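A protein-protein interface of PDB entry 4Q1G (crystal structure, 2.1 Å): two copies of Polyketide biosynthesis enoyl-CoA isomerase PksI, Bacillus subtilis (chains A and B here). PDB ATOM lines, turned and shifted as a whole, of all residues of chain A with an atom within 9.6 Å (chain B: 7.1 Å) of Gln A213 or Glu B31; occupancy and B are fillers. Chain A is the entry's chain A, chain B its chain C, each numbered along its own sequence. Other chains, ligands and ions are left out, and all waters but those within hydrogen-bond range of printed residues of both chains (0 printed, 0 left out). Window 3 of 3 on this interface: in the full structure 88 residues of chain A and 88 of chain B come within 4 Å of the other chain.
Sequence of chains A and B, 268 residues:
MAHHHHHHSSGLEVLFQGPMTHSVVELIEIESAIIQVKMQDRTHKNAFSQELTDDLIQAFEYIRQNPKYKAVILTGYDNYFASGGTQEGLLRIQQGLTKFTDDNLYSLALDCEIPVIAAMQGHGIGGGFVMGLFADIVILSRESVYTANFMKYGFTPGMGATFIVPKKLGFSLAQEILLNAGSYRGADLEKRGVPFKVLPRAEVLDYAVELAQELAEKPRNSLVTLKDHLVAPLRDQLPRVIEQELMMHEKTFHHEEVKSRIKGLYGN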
ATOM      1  N   ILE A 117      -4.041 -27.770 -12.098  1.00  0.00           N
ATOM      2  CA  ILE A 117      -4.509 -28.761 -13.107  1.00  0.00           C
ATOM      3  C   ILE A 117      -3.698 -28.599 -14.356  1.00  0.00           C
ATOM      4  O   ILE A 117      -3.678 -27.504 -14.938  1.00  0.00           O
ATOM      5  CB  ILE A 117      -5.996 -28.533 -13.474  1.00  0.00           C
ATOM      6  CG1 ILE A 117      -6.862 -28.779 -12.219  1.00  0.00           C
ATOM      7  CG2 ILE A 117      -6.456 -29.569 -14.546  1.00  0.00           C
ATOM      8  CD1 ILE A 117      -8.253 -28.071 -12.241  1.00  0.00           C
ATOM      9  N   ILE A 137      -3.556 -32.319 -10.453  1.00  0.00           N
ATOM     10  CA  ILE A 137      -4.418 -33.107 -11.319  1.00  0.00           C
ATOM     11  C   ILE A 137      -3.864 -32.987 -12.731  1.00  0.00           C
ATOM     12  O   ILE A 137      -3.676 -31.867 -13.242  1.00  0.00           O
ATOM     13  CB  ILE A 137      -5.903 -32.564 -11.272  1.00  0.00           C
ATOM     14  CG1 ILE A 137      -6.508 -32.787  -9.849  1.00  0.00           C
ATOM     15  CG2 ILE A 137      -6.775 -33.260 -12.365  1.00  0.00           C
ATOM     16  CD1 ILE A 137      -7.924 -32.230  -9.657  1.00  0.00           C
ATOM     17  N   LEU A 205      -9.901 -28.914 -22.117  1.00  0.00           N
ATOM     18  CA  LEU A 205      -9.962 -27.654 -21.414  1.00  0.00           C
ATOM     19  C   LEU A 205     -11.319 -27.450 -20.740  1.00  0.00           C
ATOM     20  O   LEU A 205     -11.382 -26.956 -19.608  1.00  0.00           O
ATOM     21  CB  LEU A 205      -9.538 -26.438 -22.328  1.00  0.00           C
ATOM     22  CG  LEU A 205      -9.373 -25.072 -21.583  1.00  0.00           C
ATOM     23  CD1 LEU A 205      -8.272 -25.162 -20.479  1.00  0.00           C
ATOM     24  CD2 LEU A 205      -9.097 -23.858 -22.472  1.00  0.00           C
ATOM     25  N   ASP A 206     -12.409 -27.833 -21.401  1.00  0.00           N
ATOM     26  CA  ASP A 206     -13.762 -27.720 -20.776  1.00  0.00           C
ATOM     27  C   ASP A 206     -13.811 -28.553 -19.502  1.00  0.00           C
ATOM     28  O   ASP A 206     -14.377 -28.152 -18.497  1.00  0.00           O
ATOM     29  CB  ASP A 206     -14.869 -28.240 -21.701  1.00  0.00           C
ATOM     30  CG  ASP A 206     -15.134 -27.308 -22.898  1.00  0.00           C
ATOM     31  OD1 ASP A 206     -14.933 -26.085 -22.740  1.00  0.00           O
ATOM     32  OD2 ASP A 206     -15.513 -27.799 -24.002  1.00  0.00           O
ATOM     33  N   TYR A 207     -13.261 -29.755 -19.576  1.00  0.00           N
ATOM     34  CA  TYR A 207     -13.303 -30.573 -18.399  1.00  0.00           C
ATOM     35  C   TYR A 207     -12.422 -29.960 -17.281  1.00  0.00           C
ATOM     36  O   TYR A 207     -12.872 -29.903 -16.071  1.00  0.00           O
ATOM     37  CB  TYR A 207     -12.847 -31.971 -18.790  1.00  0.00           C
ATOM     38  CG  TYR A 207     -12.669 -32.942 -17.646  1.00  0.00           C
ATOM     39  CD1 TYR A 207     -13.762 -33.751 -17.198  1.00  0.00           C
ATOM     40  CD2 TYR A 207     -11.443 -33.028 -16.960  1.00  0.00           C
ATOM     41  CE1 TYR A 207     -13.604 -34.615 -16.101  1.00  0.00           C
ATOM     42  CE2 TYR A 207     -11.258 -33.924 -15.910  1.00  0.00           C
ATOM     43  CZ  TYR A 207     -12.323 -34.684 -15.462  1.00  0.00           C
ATOM     44  OH  TYR A 207     -12.107 -35.555 -14.405  1.00  0.00           O
ATOM     45  N   ALA A 208     -11.206 -29.469 -17.639  1.00  0.00           N
ATOM     46  CA  ALA A 208     -10.354 -28.745 -16.632  1.00  0.00           C
ATOM     47  C   ALA A 208     -11.105 -27.587 -15.949  1.00  0.00           C
ATOM     48  O   ALA A 208     -11.029 -27.399 -14.691  1.00  0.00           O
ATOM     49  CB  ALA A 208      -9.041 -28.230 -17.249  1.00  0.00           C
ATOM     50  N   VAL A 209     -11.786 -26.777 -16.748  1.00  0.00           N
ATOM     51  CA  VAL A 209     -12.561 -25.659 -16.173  1.00  0.00           C
ATOM     52  C   VAL A 209     -13.658 -26.193 -15.237  1.00  0.00           C
ATOM     53  O   VAL A 209     -13.862 -25.678 -14.122  1.00  0.00           O
ATOM     54  CB  VAL A 209     -13.216 -24.791 -17.292  1.00  0.00           C
ATOM     55  CG1 VAL A 209     -14.186 -23.743 -16.727  1.00  0.00           C
ATOM     56  CG2 VAL A 209     -12.132 -24.104 -18.135  1.00  0.00           C
ATOM     57  N   GLU A 210     -14.373 -27.231 -15.637  1.00  0.00           N
ATOM     58  CA  GLU A 210     -15.422 -27.778 -14.686  1.00  0.00           C
ATOM     59  C   GLU A 210     -14.848 -28.275 -13.379  1.00  0.00           C
ATOM     60  O   GLU A 210     -15.427 -28.055 -12.281  1.00  0.00           O
ATOM     61  CB  GLU A 210     -16.194 -28.933 -15.324  1.00  0.00           C
ATOM     62  CG  GLU A 210     -17.005 -28.508 -16.547  1.00  0.00           C
ATOM     63  CD  GLU A 210     -17.487 -29.704 -17.404  1.00  0.00           C
ATOM     64  OE1 GLU A 210     -17.564 -30.855 -16.888  1.00  0.00           O
ATOM     65  OE2 GLU A 210     -17.804 -29.501 -18.614  1.00  0.00           O
ATOM     66  N   LEU A 211     -13.725 -28.995 -13.480  1.00  0.00           N
ATOM     67  CA  LEU A 211     -13.033 -29.457 -12.295  1.00  0.00           C
ATOM     68  C   LEU A 211     -12.554 -28.278 -11.398  1.00  0.00           C
ATOM     69  O   LEU A 211     -12.683 -28.320 -10.216  1.00  0.00           O
ATOM     70  CB  LEU A 211     -11.840 -30.289 -12.733  1.00  0.00           C
ATOM     71  CG  LEU A 211     -11.099 -31.059 -11.676  1.00  0.00           C
ATOM     72  CD1 LEU A 211     -12.058 -31.726 -10.684  1.00  0.00           C
ATOM     73  CD2 LEU A 211     -10.487 -32.192 -12.486  1.00  0.00           C
ATOM     74  N   ALA A 212     -11.920 -27.284 -12.002  1.00  0.00           N
ATOM     75  CA  ALA A 212     -11.457 -26.077 -11.341  1.00  0.00           C
ATOM     76  C   ALA A 212     -12.631 -25.342 -10.656  1.00  0.00           C
ATOM     77  O   ALA A 212     -12.484 -24.915  -9.518  1.00  0.00           O
ATOM     78  CB  ALA A 212     -10.720 -25.159 -12.341  1.00  0.00           C
ATOM     79  N   GLN A 213     -13.788 -25.261 -11.306  1.00  0.00           N
ATOM     80  CA  GLN A 213     -14.976 -24.666 -10.679  1.00  0.00           C
ATOM     81  C   GLN A 213     -15.440 -25.480  -9.444  1.00  0.00           C
ATOM     82  O   GLN A 213     -15.835 -24.916  -8.422  1.00  0.00           O
ATOM     83  CB  GLN A 213     -16.199 -24.522 -11.629  1.00  0.00           C
ATOM     84  CG  GLN A 213     -16.134 -23.571 -12.834  1.00  0.00           C
ATOM     85  CD  GLN A 213     -17.216 -23.823 -13.959  1.00  0.00           C
ATOM     86  OE1 GLN A 213     -17.456 -24.947 -14.417  1.00  0.00           O
ATOM     87  NE2 GLN A 213     -17.859 -22.765 -14.390  1.00  0.00           N
ATOM     88  N   GLU A 214     -15.401 -26.814  -9.536  1.00  0.00           N
ATOM     89  CA  GLU A 214     -15.642 -27.615  -8.365  1.00  0.00           C
ATOM     90  C   GLU A 214     -14.645 -27.440  -7.247  1.00  0.00           C
ATOM     91  O   GLU A 214     -15.041 -27.409  -6.063  1.00  0.00           O
ATOM     92  CB  GLU A 214     -15.735 -29.085  -8.743  1.00  0.00           C
ATOM     93  CG  GLU A 214     -17.040 -29.323  -9.497  1.00  0.00           C
ATOM     94  CD  GLU A 214     -17.033 -30.719 -10.129  1.00  0.00           C
ATOM     95  OE1 GLU A 214     -16.081 -31.496  -9.894  1.00  0.00           O
ATOM     96  OE2 GLU A 214     -17.930 -31.036 -10.918  1.00  0.00           O
ATOM     97  N   LEU A 215     -13.354 -27.359  -7.580  1.00  0.00           N
ATOM     98  CA  LEU A 215     -12.410 -27.066  -6.531  1.00  0.00           C
ATOM     99  C   LEU A 215     -12.657 -25.692  -5.949  1.00  0.00           C
ATOM    100  O   LEU A 215     -12.531 -25.508  -4.711  1.00  0.00           O
ATOM    101  CB  LEU A 215     -10.962 -27.100  -7.031  1.00  0.00           C
ATOM    102  CG  LEU A 215     -10.520 -28.488  -7.499  1.00  0.00           C
ATOM    103  CD1 LEU A 215      -9.297 -28.260  -8.435  1.00  0.00           C
ATOM    104  CD2 LEU A 215     -10.165 -29.270  -6.214  1.00  0.00           C
ATOM    105  N   ALA A 216     -13.035 -24.740  -6.815  1.00  0.00           N
ATOM    106  CA  ALA A 216     -13.188 -23.366  -6.336  1.00  0.00           C
ATOM    107  C   ALA A 216     -14.412 -23.223  -5.364  1.00  0.00           C
ATOM    108  O   ALA A 216     -14.628 -22.175  -4.768  1.00  0.00           O
ATOM    109  CB  ALA A 216     -13.264 -22.372  -7.507  1.00  0.00           C
ATOM    110  N   GLU A 217     -15.184 -24.300  -5.180  1.00  0.00           N
ATOM    111  CA  GLU A 217     -16.300 -24.244  -4.239  1.00  0.00           C
ATOM    112  C   GLU A 217     -15.817 -24.441  -2.796  1.00  0.00           C
ATOM    113  O   GLU A 217     -16.613 -24.361  -1.858  1.00  0.00           O
ATOM    114  CB  GLU A 217     -17.257 -25.364  -4.554  1.00  0.00           C
ATOM    115  CG  GLU A 217     -18.096 -25.096  -5.794  1.00  0.00           C
ATOM    116  CD  GLU A 217     -18.963 -26.286  -6.168  1.00  0.00           C
ATOM    117  OE1 GLU A 217     -18.911 -27.363  -5.513  1.00  0.00           O
ATOM    118  OE2 GLU A 217     -19.692 -26.139  -7.141  1.00  0.00           O
ATOM    119  N   LYS A 218     -14.533 -24.748  -2.615  1.00  0.00           N
ATOM    120  CA  LYS A 218     -14.017 -25.049  -1.297  1.00  0.00           C
ATOM    121  C   LYS A 218     -13.407 -23.789  -0.728  1.00  0.00           C
ATOM    122  O   LYS A 218     -12.925 -22.957  -1.505  1.00  0.00           O
ATOM    123  CB  LYS A 218     -12.965 -26.160  -1.406  1.00  0.00           C
ATOM    124  CG  LYS A 218     -13.550 -27.603  -1.421  1.00  0.00           C
ATOM    125  CD  LYS A 218     -14.304 -27.903  -2.726  1.00  0.00           C
ATOM    126  CE  LYS A 218     -14.336 -29.412  -2.945  1.00  0.00           C
ATOM    127  NZ  LYS A 218     -15.270 -29.595  -4.123  1.00  0.00           N
ATOM    128  N   PRO A 219     -13.381 -23.636   0.621  1.00  0.00           N
ATOM    129  CA  PRO A 219     -12.611 -22.501   1.152  1.00  0.00           C
ATOM    130  C   PRO A 219     -11.143 -22.623   0.751  1.00  0.00           C
ATOM    131  O   PRO A 219     -10.542 -23.709   0.834  1.00  0.00           O
ATOM    132  CB  PRO A 219     -12.722 -22.638   2.692  1.00  0.00           C
ATOM    133  CG  PRO A 219     -13.825 -23.659   2.926  1.00  0.00           C
ATOM    134  CD  PRO A 219     -13.930 -24.523   1.674  1.00  0.00           C
ATOM    135  N   LEU A 223      -8.284 -25.744   1.000  1.00  0.00           N
ATOM    136  CA  LEU A 223      -7.544 -26.287  -0.184  1.00  0.00           C
ATOM    137  C   LEU A 223      -6.048 -26.254   0.050  1.00  0.00           C
ATOM    138  O   LEU A 223      -5.285 -27.247  -0.271  1.00  0.00           O
ATOM    139  CB  LEU A 223      -7.897 -25.482  -1.428  1.00  0.00           C
ATOM    140  CG  LEU A 223      -9.307 -25.732  -2.004  1.00  0.00           C
ATOM    141  CD1 LEU A 223      -9.613 -24.611  -2.999  1.00  0.00           C
ATOM    142  CD2 LEU A 223      -9.565 -27.128  -2.649  1.00  0.00           C
ATOM    143  N   GLU B  29      -8.429 -15.034 -16.211  1.00  0.00           N
ATOM    144  CA  GLU B  29      -9.351 -15.407 -15.131  1.00  0.00           C
ATOM    145  C   GLU B  29     -10.603 -16.087 -15.654  1.00  0.00           C
ATOM    146  O   GLU B  29     -11.186 -15.670 -16.637  1.00  0.00           O
ATOM    147  CB  GLU B  29      -9.779 -14.209 -14.229  1.00  0.00           C
ATOM    148  CG  GLU B  29      -8.537 -13.531 -13.630  1.00  0.00           C
ATOM    149  CD  GLU B  29      -8.874 -12.551 -12.507  1.00  0.00           C
ATOM    150  OE1 GLU B  29     -10.054 -12.212 -12.318  1.00  0.00           O
ATOM    151  OE2 GLU B  29      -7.946 -12.107 -11.798  1.00  0.00           O
ATOM    152  N   ILE B  30     -11.025 -17.134 -14.938  1.00  0.00           N
ATOM    153  CA  ILE B  30     -12.234 -17.808 -15.268  1.00  0.00           C
ATOM    154  C   ILE B  30     -13.113 -17.725 -14.055  1.00  0.00           C
ATOM    155  O   ILE B  30     -12.657 -17.994 -12.949  1.00  0.00           O
ATOM    156  CB  ILE B  30     -11.968 -19.286 -15.694  1.00  0.00           C
ATOM    157  CG1 ILE B  30     -11.277 -19.273 -17.050  1.00  0.00           C
ATOM    158  CG2 ILE B  30     -13.289 -20.022 -15.775  1.00  0.00           C
ATOM    159  CD1 ILE B  30     -10.380 -20.461 -17.302  1.00  0.00           C
ATOM    160  N   GLU B  31     -14.358 -17.336 -14.261  1.00  0.00           N
ATOM    161  CA  GLU B  31     -15.282 -17.087 -13.121  1.00  0.00           C
ATOM    162  C   GLU B  31     -14.574 -16.148 -12.075  1.00  0.00           C
ATOM    163  O   GLU B  31     -13.876 -15.222 -12.474  1.00  0.00           O
ATOM    164  CB  GLU B  31     -15.630 -18.415 -12.475  1.00  0.00           C
ATOM    165  CG  GLU B  31     -16.305 -19.410 -13.371  1.00  0.00           C
ATOM    166  CD  GLU B  31     -17.789 -19.144 -13.573  1.00  0.00           C
ATOM    167  OE1 GLU B  31     -18.407 -18.319 -12.851  1.00  0.00           O
ATOM    168  OE2 GLU B  31     -18.359 -19.780 -14.470  1.00  0.00           O
ATOM    169  N   SER B  32     -14.695 -16.415 -10.770  1.00  0.00           N
ATOM    170  CA  SER B  32     -14.093 -15.586  -9.729  1.00  0.00           C
ATOM    171  C   SER B  32     -12.672 -15.942  -9.350  1.00  0.00           C
ATOM    172  O   SER B  32     -11.880 -15.040  -9.122  1.00  0.00           O
ATOM    173  CB  SER B  32     -14.848 -15.727  -8.420  1.00  0.00           C
ATOM    174  OG  SER B  32     -16.073 -15.033  -8.534  1.00  0.00           O
ATOM    175  N   ALA B  33     -12.357 -17.231  -9.241  1.00  0.00           N
ATOM    176  CA  ALA B  33     -11.169 -17.611  -8.512  1.00  0.00           C
ATOM    177  C   ALA B  33     -10.338 -18.638  -9.222  1.00  0.00           C
ATOM    178  O   ALA B  33      -9.525 -19.273  -8.579  1.00  0.00           O
ATOM    179  CB  ALA B  33     -11.546 -18.131  -7.114  1.00  0.00           C
ATOM    180  N   ILE B  34     -10.511 -18.763 -10.548  1.00  0.00           N
ATOM    181  CA  ILE B  34      -9.775 -19.709 -11.339  1.00  0.00           C
ATOM    182  C   ILE B  34      -8.830 -18.903 -12.220  1.00  0.00           C
ATOM    183  O   ILE B  34      -9.205 -17.918 -12.837  1.00  0.00           O
ATOM    184  CB  ILE B  34     -10.652 -20.549 -12.241  1.00  0.00           C
ATOM    185  CG1 ILE B  34     -11.606 -21.394 -11.405  1.00  0.00           C
ATOM    186  CG2 ILE B  34      -9.786 -21.395 -13.195  1.00  0.00           C
ATOM    187  CD1 ILE B  34     -12.755 -21.929 -12.273  1.00  0.00           C
ATOM    188  N   LYS B  68      -6.625 -14.278  -4.150  1.00  0.00           N
ATOM    189  CA  LYS B  68      -7.933 -14.552  -4.727  1.00  0.00           C
ATOM    190  C   LYS B  68      -8.016 -15.965  -5.313  1.00  0.00           C
ATOM    191  O   LYS B  68      -9.020 -16.581  -5.257  1.00  0.00           O
ATOM    192  CB  LYS B  68      -8.245 -13.526  -5.836  1.00  0.00           C
ATOM    193  CG  LYS B  68      -9.430 -13.875  -6.735  1.00  0.00           C
ATOM    194  CD  LYS B  68      -9.925 -12.680  -7.600  1.00  0.00           C
ATOM    195  CE  LYS B  68      -8.970 -12.374  -8.734  1.00  0.00           C
ATOM    196  NZ  LYS B  68      -9.435 -11.328  -9.694  1.00  0.00           N
ATOM    197  N   ALA B  71      -7.717 -22.055  -7.850  1.00  0.00           N
ATOM    198  CA  ALA B  71      -7.177 -23.154  -8.679  1.00  0.00           C
ATOM    199  C   ALA B  71      -6.533 -22.595  -9.934  1.00  0.00           C
ATOM    200  O   ALA B  71      -6.957 -21.555 -10.421  1.00  0.00           O
ATOM    201  CB  ALA B  71      -8.270 -24.151  -9.049  1.00  0.00           C
ATOM    202  N   ILE B  73      -5.260 -23.471 -13.904  1.00  0.00           N
ATOM    203  CA  ILE B  73      -5.254 -24.382 -15.071  1.00  0.00           C
ATOM    204  C   ILE B  73      -4.011 -24.044 -15.921  1.00  0.00           C
ATOM    205  O   ILE B  73      -3.902 -22.931 -16.433  1.00  0.00           O
ATOM    206  CB  ILE B  73      -6.541 -24.326 -15.950  1.00  0.00           C
ATOM    207  CG1 ILE B  73      -7.806 -24.602 -15.038  1.00  0.00           C
ATOM    208  CG2 ILE B  73      -6.444 -25.359 -17.103  1.00  0.00           C
ATOM    209  CD1 ILE B  73      -9.158 -24.339 -15.738  1.00  0.00           C
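The side-chain carboxylate (OE2) of Glu B31 is in hydrogen-bond range of the side-chain amide nitrogen (NE2) of Gln A213, 3.0 Å away.
Ile A117 touches Ile B73 (O to CA, 3.5 Å). Ile B73 touches Leu A205. CD1 of Ile B73 touches O of Ala A208, 3.7 Å away. CG2 of Ile B30 touches CG1 of Val A209 (3.9 Å). Val A209 touches Ile B73 (CA to CD1, 3.7 Å). Ile B34 touches Ala A212. Ala A212 touches Ile B73. CD1 of Ile B34 touches N of Gln A213 (3.6 Å).
Of the printed residues of chain B, Ile A117 touches Ile B73 (3.5 Å). Ile A137 touches none of the printed residues of chain B. Printed residues of chain B within 4 Å of Leu A205: Ile B73. Printed residues of chain B within 4 Å of Ala A208: Ile B73 (3.7 Å). Of chain B, only Glu B31 (3.0 Å) and Ile B34 (3.6 Å) come within 4 Å of Gln A213. Leu A215 touches none of the printed residues of chain B. Of the printed residues of chain A, Ile B30 touches Val A209 (3.9 Å). Glu B31 touches just one residue of chain A: Gln A213 (3.0 Å). Of the printed residues of chain A, Ile B34 touches Ala A212 and Gln A213. The nearest printed residue of chain A that does not touch Ile B34 is Val A209 (4.3 Å).
Of the 9 printed residues of chain B, 4 touch a printed residue of chain A. Hydrophobic or aromatic side chains of chain B that line the printed part of chain A: Ile B30, Ile B34 and Ile B73. Hydrophobic or aromatic side chains of chain A within 4 Å of the printed part of chain B: Leu A205, Ala A208, Val A209 and Ala A212. Along chain A the printed residues that touch a printed residue of chain B span positions 117 to 213. Among the printed residues, 9 pairs touch across the chains.
No position is printed for both chains. Of the 9 pairs that touch across the chains among the printed residues, none has its exchanged pair printed and touching as well.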
